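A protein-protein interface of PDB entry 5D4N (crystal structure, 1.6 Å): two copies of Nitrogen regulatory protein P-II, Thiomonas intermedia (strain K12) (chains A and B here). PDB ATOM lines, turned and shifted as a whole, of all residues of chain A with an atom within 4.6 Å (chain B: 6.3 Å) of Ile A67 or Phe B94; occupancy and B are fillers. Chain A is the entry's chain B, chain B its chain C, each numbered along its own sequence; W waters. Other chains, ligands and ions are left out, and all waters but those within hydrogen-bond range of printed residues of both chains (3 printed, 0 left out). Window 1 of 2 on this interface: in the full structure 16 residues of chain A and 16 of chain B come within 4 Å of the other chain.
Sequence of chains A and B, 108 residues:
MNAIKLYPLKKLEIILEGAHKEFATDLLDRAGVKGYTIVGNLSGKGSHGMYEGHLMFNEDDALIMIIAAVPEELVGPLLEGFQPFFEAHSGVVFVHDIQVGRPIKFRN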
ATOM      1  N   LYS A  11      -3.035  -1.390  12.312  1.00  0.00           N
ATOM      2  CA  LYS A  11      -4.317  -2.004  11.998  1.00  0.00           C
ATOM      3  C   LYS A  11      -4.312  -2.353  10.530  1.00  0.00           C
ATOM      4  O   LYS A  11      -4.134  -1.473   9.704  1.00  0.00           O
ATOM      5  CB  LYS A  11      -5.490  -1.087  12.312  1.00  0.00           C
ATOM      6  CG  LYS A  11      -6.829  -1.856  12.302  1.00  0.00           C
ATOM      7  CD  LYS A  11      -8.017  -0.937  12.183  1.00  0.00           C
ATOM      8  CE  LYS A  11      -8.212  -0.499  10.791  1.00  0.00           C
ATOM      9  NZ  LYS A  11      -9.416   0.366  10.650  1.00  0.00           N
ATOM     10  N   LEU A  12      -4.501  -3.635  10.241  1.00  0.00           N
ATOM     11  CA  LEU A  12      -4.554  -4.087   8.856  1.00  0.00           C
ATOM     12  C   LEU A  12      -5.994  -4.166   8.426  1.00  0.00           C
ATOM     13  O   LEU A  12      -6.849  -4.625   9.194  1.00  0.00           O
ATOM     14  CB  LEU A  12      -3.978  -5.511   8.749  1.00  0.00           C
ATOM     15  CG  LEU A  12      -2.557  -5.760   9.261  1.00  0.00           C
ATOM     16  CD1 LEU A  12      -2.134  -7.225   9.015  1.00  0.00           C
ATOM     17  CD2 LEU A  12      -1.597  -4.774   8.614  1.00  0.00           C
ATOM     18  N   GLU A  13      -6.245  -3.780   7.172  1.00  0.00           N
ATOM     19  CA  GLU A  13      -7.528  -3.973   6.495  1.00  0.00           C
ATOM     20  C   GLU A  13      -7.132  -4.858   5.321  1.00  0.00           C
ATOM     21  O   GLU A  13      -6.310  -4.455   4.496  1.00  0.00           O
ATOM     22  CB  GLU A  13      -8.164  -2.672   6.017  1.00  0.00           C
ATOM     23  CG  GLU A  13      -8.715  -1.882   7.197  1.00  0.00           C
ATOM     24  CD  GLU A  13      -9.322  -0.535   6.842  1.00  0.00           C
ATOM     25  OE1 GLU A  13      -9.172  -0.068   5.686  1.00  0.00           O
ATOM     26  OE2 GLU A  13      -9.941   0.072   7.743  1.00  0.00           O
ATOM     27  N   TYR A  36      -9.670 -10.871  15.289  1.00  0.00           N
ATOM     28  CA  TYR A  36      -9.920 -10.184  14.028  1.00  0.00           C
ATOM     29  C   TYR A  36     -11.415  -9.958  13.907  1.00  0.00           C
ATOM     30  O   TYR A  36     -12.194 -10.613  14.624  1.00  0.00           O
ATOM     31  CB  TYR A  36      -9.342 -10.961  12.814  1.00  0.00           C
ATOM     32  CG  TYR A  36      -9.830 -12.388  12.708  1.00  0.00           C
ATOM     33  CD1 TYR A  36     -11.113 -12.676  12.244  1.00  0.00           C
ATOM     34  CD2 TYR A  36      -9.007 -13.453  13.051  1.00  0.00           C
ATOM     35  CE1 TYR A  36     -11.575 -13.992  12.149  1.00  0.00           C
ATOM     36  CE2 TYR A  36      -9.446 -14.770  12.938  1.00  0.00           C
ATOM     37  CZ  TYR A  36     -10.742 -15.036  12.514  1.00  0.00           C
ATOM     38  OH  TYR A  36     -11.173 -16.346  12.417  1.00  0.00           O
ATOM     39  N   THR A  37     -11.808  -9.041  13.035  1.00  0.00           N
ATOM     40  CA  THR A  37     -13.193  -8.710  12.774  1.00  0.00           C
ATOM     41  C   THR A  37     -13.386  -8.776  11.260  1.00  0.00           C
ATOM     42  O   THR A  37     -12.536  -8.304  10.513  1.00  0.00           O
ATOM     43  CB  THR A  37     -13.467  -7.271  13.295  1.00  0.00           C
ATOM     44  OG1 THR A  37     -13.300  -7.309  14.710  1.00  0.00           O
ATOM     45  CG2 THR A  37     -14.892  -6.815  12.988  1.00  0.00           C
ATOM     46  N   VAL A  39     -15.779  -7.765   8.002  1.00  0.00           N
ATOM     47  CA  VAL A  39     -16.867  -6.989   7.407  1.00  0.00           C
ATOM     48  C   VAL A  39     -17.244  -7.744   6.138  1.00  0.00           C
ATOM     49  O   VAL A  39     -16.426  -7.888   5.228  1.00  0.00           O
ATOM     50  CB  VAL A  39     -16.436  -5.534   7.075  1.00  0.00           C
ATOM     51  CG1 VAL A  39     -17.642  -4.732   6.581  1.00  0.00           C
ATOM     52  CG2 VAL A  39     -15.766  -4.864   8.283  1.00  0.00           C
ATOM     53  N   MET A  65     -13.741  -7.852   4.176  1.00  0.00           N
ATOM     54  CA  MET A  65     -12.612  -7.078   4.698  1.00  0.00           C
ATOM     55  C   MET A  65     -12.325  -7.601   6.079  1.00  0.00           C
ATOM     56  O   MET A  65     -13.215  -7.579   6.952  1.00  0.00           O
ATOM     57  CB  MET A  65     -12.912  -5.568   4.739  1.00  0.00           C
ATOM     58  CG  MET A  65     -11.749  -4.802   5.356  1.00  0.00           C
ATOM     59  SD  MET A  65     -11.977  -2.962   5.142  1.00  0.00           S
ATOM     60  CE  MET A  65     -13.392  -2.691   6.175  1.00  0.00           C
ATOM     61  N   ILE A  66     -11.104  -8.095   6.280  1.00  0.00           N
ATOM     62  CA  ILE A  66     -10.699  -8.616   7.591  1.00  0.00           C
ATOM     63  C   ILE A  66      -9.903  -7.525   8.251  1.00  0.00           C
ATOM     64  O   ILE A  66      -8.946  -7.017   7.658  1.00  0.00           O
ATOM     65  CB  ILE A  66      -9.851  -9.886   7.439  1.00  0.00           C
ATOM     66  CG1 ILE A  66     -10.655 -10.993   6.728  1.00  0.00           C
ATOM     67  CG2 ILE A  66      -9.393 -10.357   8.855  1.00  0.00           C
ATOM     68  CD1 ILE A  66      -9.814 -12.233   6.304  1.00  0.00           C
ATOM     69  N   ILE A  67     -10.307  -7.156   9.477  1.00  0.00           N
ATOM     70  CA  ILE A  67      -9.644  -6.071  10.218  1.00  0.00           C
ATOM     71  C   ILE A  67      -8.872  -6.754  11.344  1.00  0.00           C
ATOM     72  O   ILE A  67      -9.463  -7.513  12.133  1.00  0.00           O
ATOM     73  CB  ILE A  67     -10.678  -5.087  10.824  1.00  0.00           C
ATOM     74  CG1 ILE A  67     -11.540  -4.402   9.733  1.00  0.00           C
ATOM     75  CG2 ILE A  67      -9.962  -4.044  11.743  1.00  0.00           C
ATOM     76  CD1 ILE A  67     -12.785  -3.663  10.293  1.00  0.00           C
ATOM     77  N   ALA A  68      -7.572  -6.462  11.447  1.00  0.00           N
ATOM     78  CA  ALA A  68      -6.763  -7.023  12.538  1.00  0.00           C
ATOM     79  C   ALA A  68      -5.866  -5.932  13.095  1.00  0.00           C
ATOM     80  O   ALA A  68      -5.181  -5.291  12.321  1.00  0.00           O
ATOM     81  CB  ALA A  68      -5.922  -8.182  12.041  1.00  0.00           C
ATOM     82  N   ALA A  69      -5.806  -5.780  14.434  1.00  0.00           N
ATOM     83  CA  ALA A  69      -4.910  -4.797  15.045  1.00  0.00           C
ATOM     84  C   ALA A  69      -3.803  -5.619  15.649  1.00  0.00           C
ATOM     85  O   ALA A  69      -4.044  -6.546  16.429  1.00  0.00           O
ATOM     86  CB  ALA A  69      -5.626  -4.007  16.125  1.00  0.00           C
ATOM     87  N   ILE A  98      -2.589   3.063  14.454  1.00  0.00           N
ATOM     88  CA  ILE A  98      -3.699   3.402  15.347  1.00  0.00           C
ATOM     89  C   ILE A  98      -3.159   3.417  16.768  1.00  0.00           C
ATOM     90  O   ILE A  98      -2.010   3.020  17.016  1.00  0.00           O
ATOM     91  CB  ILE A  98      -4.889   2.376  15.246  1.00  0.00           C
ATOM     92  CG1 ILE A  98      -4.424   0.948  15.610  1.00  0.00           C
ATOM     93  CG2 ILE A  98      -5.573   2.397  13.854  1.00  0.00           C
ATOM     94  CD1 ILE A  98      -5.551  -0.024  16.049  1.00  0.00           C
ATOM     95  N   GLN A  99      -4.008   3.853  17.693  1.00  0.00           N
ATOM     96  CA  GLN A  99      -3.707   3.811  19.110  1.00  0.00           C
ATOM     97  C   GLN A  99      -4.843   3.073  19.783  1.00  0.00           C
ATOM     98  O   GLN A  99      -5.985   3.114  19.316  1.00  0.00           O
ATOM     99  CB  GLN A  99      -3.562   5.213  19.703  1.00  0.00           C
ATOM    100  CG  GLN A  99      -2.350   5.964  19.192  1.00  0.00           C
ATOM    101  CD  GLN A  99      -2.306   7.329  19.810  1.00  0.00           C
ATOM    102  OE1 GLN A  99      -3.005   8.252  19.378  1.00  0.00           O
ATOM    103  NE2 GLN A  99      -1.516   7.473  20.854  1.00  0.00           N
ATOM    104  N   VAL A 100      -4.524   2.368  20.869  1.00  0.00           N
ATOM    105  CA  VAL A 100      -5.530   1.632  21.647  1.00  0.00           C
ATOM    106  C   VAL A 100      -5.270   1.960  23.117  1.00  0.00           C
ATOM    107  O   VAL A 100      -4.106   2.148  23.496  1.00  0.00           O
ATOM    108  CB  VAL A 100      -5.502   0.097  21.365  1.00  0.00           C
ATOM    109  CG1 VAL A 100      -5.966  -0.206  19.935  1.00  0.00           C
ATOM    110  CG2 VAL A 100      -4.120  -0.524  21.649  1.00  0.00           C
ATOM    111  N   LYS B  11     -10.487   9.615  14.761  1.00  0.00           N
ATOM    112  CA  LYS B  11     -11.622   8.801  14.349  1.00  0.00           C
ATOM    113  C   LYS B  11     -11.603   7.523  15.146  1.00  0.00           C
ATOM    114  O   LYS B  11     -10.608   6.798  15.125  1.00  0.00           O
ATOM    115  CB  LYS B  11     -11.577   8.479  12.852  1.00  0.00           C
ATOM    116  CG  LYS B  11     -12.919   7.919  12.306  1.00  0.00           C
ATOM    117  CD  LYS B  11     -12.749   7.186  11.009  1.00  0.00           C
ATOM    118  CE  LYS B  11     -12.206   5.789  11.239  1.00  0.00           C
ATOM    119  NZ  LYS B  11     -11.997   5.066   9.957  1.00  0.00           N
ATOM    120  N   LEU B  12     -12.681   7.275  15.884  1.00  0.00           N
ATOM    121  CA  LEU B  12     -12.802   6.021  16.620  1.00  0.00           C
ATOM    122  C   LEU B  12     -13.485   4.967  15.790  1.00  0.00           C
ATOM    123  O   LEU B  12     -14.428   5.277  15.044  1.00  0.00           O
ATOM    124  CB  LEU B  12     -13.633   6.218  17.893  1.00  0.00           C
ATOM    125  CG  LEU B  12     -13.197   7.338  18.828  1.00  0.00           C
ATOM    126  CD1 LEU B  12     -14.008   7.297  20.093  1.00  0.00           C
ATOM    127  CD2 LEU B  12     -11.722   7.232  19.215  1.00  0.00           C
ATOM    128  N   GLU B  13     -13.038   3.722  15.912  1.00  0.00           N
ATOM    129  CA  GLU B  13     -13.725   2.535  15.408  1.00  0.00           C
ATOM    130  C   GLU B  13     -14.027   1.726  16.663  1.00  0.00           C
ATOM    131  O   GLU B  13     -13.099   1.308  17.351  1.00  0.00           O
ATOM    132  CB  GLU B  13     -12.884   1.710  14.433  1.00  0.00           C
ATOM    133  CG  GLU B  13     -12.778   2.451  13.120  1.00  0.00           C
ATOM    134  CD  GLU B  13     -11.932   1.798  12.049  1.00  0.00           C
ATOM    135  OE1 GLU B  13     -11.245   0.791  12.350  1.00  0.00           O
ATOM    136  OE2 GLU B  13     -11.958   2.305  10.894  1.00  0.00           O
ATOM    137  N   ILE B  14     -15.295   1.619  17.037  1.00  0.00           N
ATOM    138  CA  ILE B  14     -15.686   0.925  18.279  1.00  0.00           C
ATOM    139  C   ILE B  14     -16.349  -0.366  17.862  1.00  0.00           C
ATOM    140  O   ILE B  14     -17.417  -0.320  17.263  1.00  0.00           O
ATOM    141  CB  ILE B  14     -16.640   1.804  19.091  1.00  0.00           C
ATOM    142  CG1 ILE B  14     -15.990   3.179  19.382  1.00  0.00           C
ATOM    143  CG2 ILE B  14     -17.083   1.065  20.370  1.00  0.00           C
ATOM    144  CD1 ILE B  14     -17.025   4.323  19.678  1.00  0.00           C
ATOM    145  N   ILE B  15     -15.734  -1.508  18.181  1.00  0.00           N
ATOM    146  CA  ILE B  15     -16.287  -2.797  17.745  1.00  0.00           C
ATOM    147  C   ILE B  15     -16.841  -3.494  18.963  1.00  0.00           C
ATOM    148  O   ILE B  15     -16.125  -3.675  19.954  1.00  0.00           O
ATOM    149  CB  ILE B  15     -15.223  -3.665  17.019  1.00  0.00           C
ATOM    150  CG1 ILE B  15     -14.700  -2.930  15.764  1.00  0.00           C
ATOM    151  CG2 ILE B  15     -15.823  -5.031  16.658  1.00  0.00           C
ATOM    152  CD1 ILE B  15     -13.397  -3.526  15.188  1.00  0.00           C
ATOM    153  N   LEU B  42     -21.272  -7.610  11.409  1.00  0.00           N
ATOM    154  CA  LEU B  42     -19.861  -8.000  11.408  1.00  0.00           C
ATOM    155  C   LEU B  42     -19.754  -9.310  12.190  1.00  0.00           C
ATOM    156  O   LEU B  42     -20.636  -9.629  12.963  1.00  0.00           O
ATOM    157  CB  LEU B  42     -18.993  -6.963  12.123  1.00  0.00           C
ATOM    158  CG  LEU B  42     -19.022  -5.528  11.572  1.00  0.00           C
ATOM    159  CD1 LEU B  42     -17.814  -4.809  12.012  1.00  0.00           C
ATOM    160  CD2 LEU B  42     -19.108  -5.506  10.053  1.00  0.00           C
ATOM    161  N   HIS B  48      -8.618  -8.344  19.685  1.00  0.00           N
ATOM    162  CA  HIS B  48      -7.678  -7.488  18.963  1.00  0.00           C
ATOM    163  C   HIS B  48      -6.421  -7.073  19.740  1.00  0.00           C
ATOM    164  O   HIS B  48      -6.503  -6.604  20.872  1.00  0.00           O
ATOM    165  CB  HIS B  48      -8.418  -6.286  18.428  1.00  0.00           C
ATOM    166  CG  HIS B  48      -9.146  -6.577  17.152  1.00  0.00           C
ATOM    167  ND1 HIS B  48      -8.453  -6.833  15.980  1.00  0.00           N
ATOM    168  CD2 HIS B  48     -10.479  -6.621  16.895  1.00  0.00           C
ATOM    169  CE1 HIS B  48      -9.379  -6.958  15.037  1.00  0.00           C
ATOM    170  NE2 HIS B  48     -10.615  -6.848  15.532  1.00  0.00           N
ATOM    171  N   MET B  65     -19.624  -2.175  14.142  1.00  0.00           N
ATOM    172  CA  MET B  65     -18.516  -1.236  14.291  1.00  0.00           C
ATOM    173  C   MET B  65     -19.101   0.165  14.221  1.00  0.00           C
ATOM    174  O   MET B  65     -19.756   0.514  13.220  1.00  0.00           O
ATOM    175  CB  MET B  65     -17.445  -1.437  13.222  1.00  0.00           C
ATOM    176  CG  MET B  65     -16.333  -0.421  13.354  1.00  0.00           C
ATOM    177  SD  MET B  65     -14.925  -0.744  12.206  1.00  0.00           S
ATOM    178  CE  MET B  65     -15.693  -0.544  10.672  1.00  0.00           C
ATOM    179  N   VAL B  92     -13.554  -3.539  21.377  1.00  0.00           N
ATOM    180  CA  VAL B  92     -12.376  -2.689  21.374  1.00  0.00           C
ATOM    181  C   VAL B  92     -12.669  -1.313  20.786  1.00  0.00           C
ATOM    182  O   VAL B  92     -13.602  -1.178  19.993  1.00  0.00           O
ATOM    183  CB  VAL B  92     -11.281  -3.416  20.535  1.00  0.00           C
ATOM    184  CG1 VAL B  92     -11.639  -3.502  19.044  1.00  0.00           C
ATOM    185  CG2 VAL B  92      -9.894  -2.806  20.747  1.00  0.00           C
ATOM    186  N   VAL B  93     -11.799  -0.332  21.076  1.00  0.00           N
ATOM    187  CA  VAL B  93     -11.849   0.995  20.419  1.00  0.00           C
ATOM    188  C   VAL B  93     -10.487   1.219  19.715  1.00  0.00           C
ATOM    189  O   VAL B  93      -9.464   1.176  20.403  1.00  0.00           O
ATOM    190  CB  VAL B  93     -12.118   2.180  21.374  1.00  0.00           C
ATOM    191  CG1 VAL B  93     -12.156   3.500  20.582  1.00  0.00           C
ATOM    192  CG2 VAL B  93     -13.404   1.990  22.182  1.00  0.00           C
ATOM    193  N   PHE B  94     -10.464   1.434  18.381  1.00  0.00           N
ATOM    194  CA  PHE B  94      -9.241   1.790  17.667  1.00  0.00           C
ATOM    195  C   PHE B  94      -9.304   3.304  17.445  1.00  0.00           C
ATOM    196  O   PHE B  94     -10.298   3.792  16.893  1.00  0.00           O
ATOM    197  CB  PHE B  94      -9.170   1.118  16.298  1.00  0.00           C
ATOM    198  CG  PHE B  94      -9.226  -0.384  16.302  1.00  0.00           C
ATOM    199  CD1 PHE B  94      -8.638  -1.121  17.335  1.00  0.00           C
ATOM    200  CD2 PHE B  94      -9.820  -1.076  15.245  1.00  0.00           C
ATOM    201  CE1 PHE B  94      -8.621  -2.516  17.296  1.00  0.00           C
ATOM    202  CE2 PHE B  94      -9.828  -2.476  15.229  1.00  0.00           C
ATOM    203  CZ  PHE B  94      -9.243  -3.187  16.260  1.00  0.00           C
ATOM    204  N   VAL B  95      -8.247   4.018  17.793  1.00  0.00           N
ATOM    205  CA  VAL B  95      -8.179   5.467  17.610  1.00  0.00           C
ATOM    206  C   VAL B  95      -7.301   5.763  16.412  1.00  0.00           C
ATOM    207  O   VAL B  95      -6.126   5.380  16.412  1.00  0.00           O
ATOM    208  CB  VAL B  95      -7.653   6.211  18.868  1.00  0.00           C
ATOM    209  CG1 VAL B  95      -7.751   7.734  18.685  1.00  0.00           C
ATOM    210  CG2 VAL B  95      -8.374   5.759  20.148  1.00  0.00           C
ATOM    211  N   HIS B  96      -7.846   6.464  15.422  1.00  0.00           N
ATOM    212  CA  HIS B  96      -7.092   6.833  14.224  1.00  0.00           C
ATOM    213  C   HIS B  96      -6.870   8.345  14.180  1.00  0.00           C
ATOM    214  O   HIS B  96      -7.695   9.128  14.686  1.00  0.00           O
ATOM    215  CB  HIS B  96      -7.927   6.524  12.963  1.00  0.00           C
ATOM    216  CG  HIS B  96      -8.233   5.092  12.733  1.00  0.00           C
ATOM    217  ND1 HIS B  96      -9.131   4.431  13.519  1.00  0.00           N
ATOM    218  CD2 HIS B  96      -7.776   4.262  11.761  1.00  0.00           C
ATOM    219  CE1 HIS B  96      -9.176   3.195  13.046  1.00  0.00           C
ATOM    220  NE2 HIS B  96      -8.417   3.058  11.967  1.00  0.00           N
HETATM  221  O   HOH W   1     -12.237  -0.533   8.887  1.00  0.00           O
HETATM  222  O   HOH W   2      -4.344   7.648  16.929  1.00  0.00           O
HETATM  223  O   HOH W   3     -10.251   2.800   8.707  1.00  0.00           O
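The side-chain carboxylate of Glu B13 lies within salt-bridge range of the side-chain amino group of Lys B11 (2.9 Å).
The backbone carbonyl oxygen of Glu B13 lies within hydrogen-bond range of the backbone NH of Phe B94, 2.8 Å away.
The backbone NH (N) of Val A39 is in hydrogen-bond range of the backbone carbonyl oxygen (O) of Met A65.
The backbone NH of His B96 lies within hydrogen-bond range of the backbone carbonyl oxygen of Lys B11, at 2.8 Å.
OE2 of Glu A13 is in salt-bridge range of NZ of Lys A11 (3.0 Å).
The backbone NH (N) of Ile B15 is in hydrogen-bond range of the backbone carbonyl oxygen (O) of Val B92, at 2.8 Å.
Of the 14 printed residues of chain A, 10 touch a printed residue of chain B.
Hydrophobic or aromatic side chains of chain A that line the printed part of chain B: Val A39, Ile A67, Ala A69, Ile A98 and Val A100.
Along chain B the printed residues that touch a printed residue of chain A span positions 13 to 96.
Among the printed residues, Asp or Glu carboxylates within 4 Å of a Lys or Arg side-chain nitrogen of the other chain: Lys A11 with Glu B13 (2.5 Å).
Lys A11 touches Phe B94.
His B48 touches Tyr A36.
OG1 of Thr A37 touches CD1 of Ile B15 (3.8 Å).
Thr A37 touches Leu B42.
CD2 of Leu B42 touches CA of Val A39, at 3.8 Å.
CB of Ala A69 touches CE1 of Phe B94, 3.5 Å away.
Ile A98 touches Val B95.
CG2 of Ile A98 touches NE2 of His B96, at 3.5 Å.
Gln A99 touches Phe B94.
Val B93 touches Val A100.
Water W1 lies within hydrogen-bond range of OE2 of Glu A13 (2.6 Å), NZ of Lys A11 (3.4 Å) and OE2 of Glu B13 (3.5 Å).
Water W3 lies within hydrogen-bond range of OE2 of Glu B13 (2.8 Å), OE2 of Glu A13 (2.9 Å), NZ of Lys B11 (3.1 Å) and NZ of Lys A11 (3.2 Å).
Water W2 lies within hydrogen-bond range of the side-chain amide oxygen (OE1) of Gln A99 (2.9 Å) and the backbone carbonyl oxygen (O) of Val B95 (2.9 Å).
Lys A11 touches Glu B13, but with the chains exchanged Glu A13 does not touch Lys B11 (5.8 Å).
Of the 20 pairs that touch across the chains among the printed residues, none has its exchanged pair printed and touching as well.
Ile A67 touches two residues of chain B.
Printed residues of chain B within 4 Å of Ile A98: Phe B94 (3.5 Å), Val B95 (3.3 Å) and His B96 (3.5 Å).
Of the printed residues of chain A, Val B93 touches Val A100 (3.8 Å).
Printed residues of chain B within 4 Å of Ala A68: His B48 (3.6 Å).
Of the printed residues of chain A, Leu B42 touches Thr A37 (3.7 Å) and Val A39 (3.8 Å).
Ile B14 touches none of the printed residues of chain A.
The nearest residue of chain B that does not touch Ile A67 is Met B65 (4.1 Å).
The side-chain amino group (NZ) of Lys A11 is in hydrogen-bond range of a ring nitrogen (NE2) of His B96, at 3.2 Å.
A ring nitrogen (NE2) of His B48 is in hydrogen-bond range of the side-chain hydroxyl (OG1) of Thr A37, 2.8 Å away.
The backbone NH (N) of Val B95 sits at hydrogen-bond distance from the backbone carbonyl oxygen (O) of Gln A99 (2.9 Å).
The backbone NH (N) of Ala A69 is in hydrogen-bond range of a ring nitrogen (ND1) of His B48 (3.2 Å).
The side-chain amino group (NZ) of Lys A11 lies within salt-bridge range of the side-chain carboxylate (OE1) of Glu B13.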
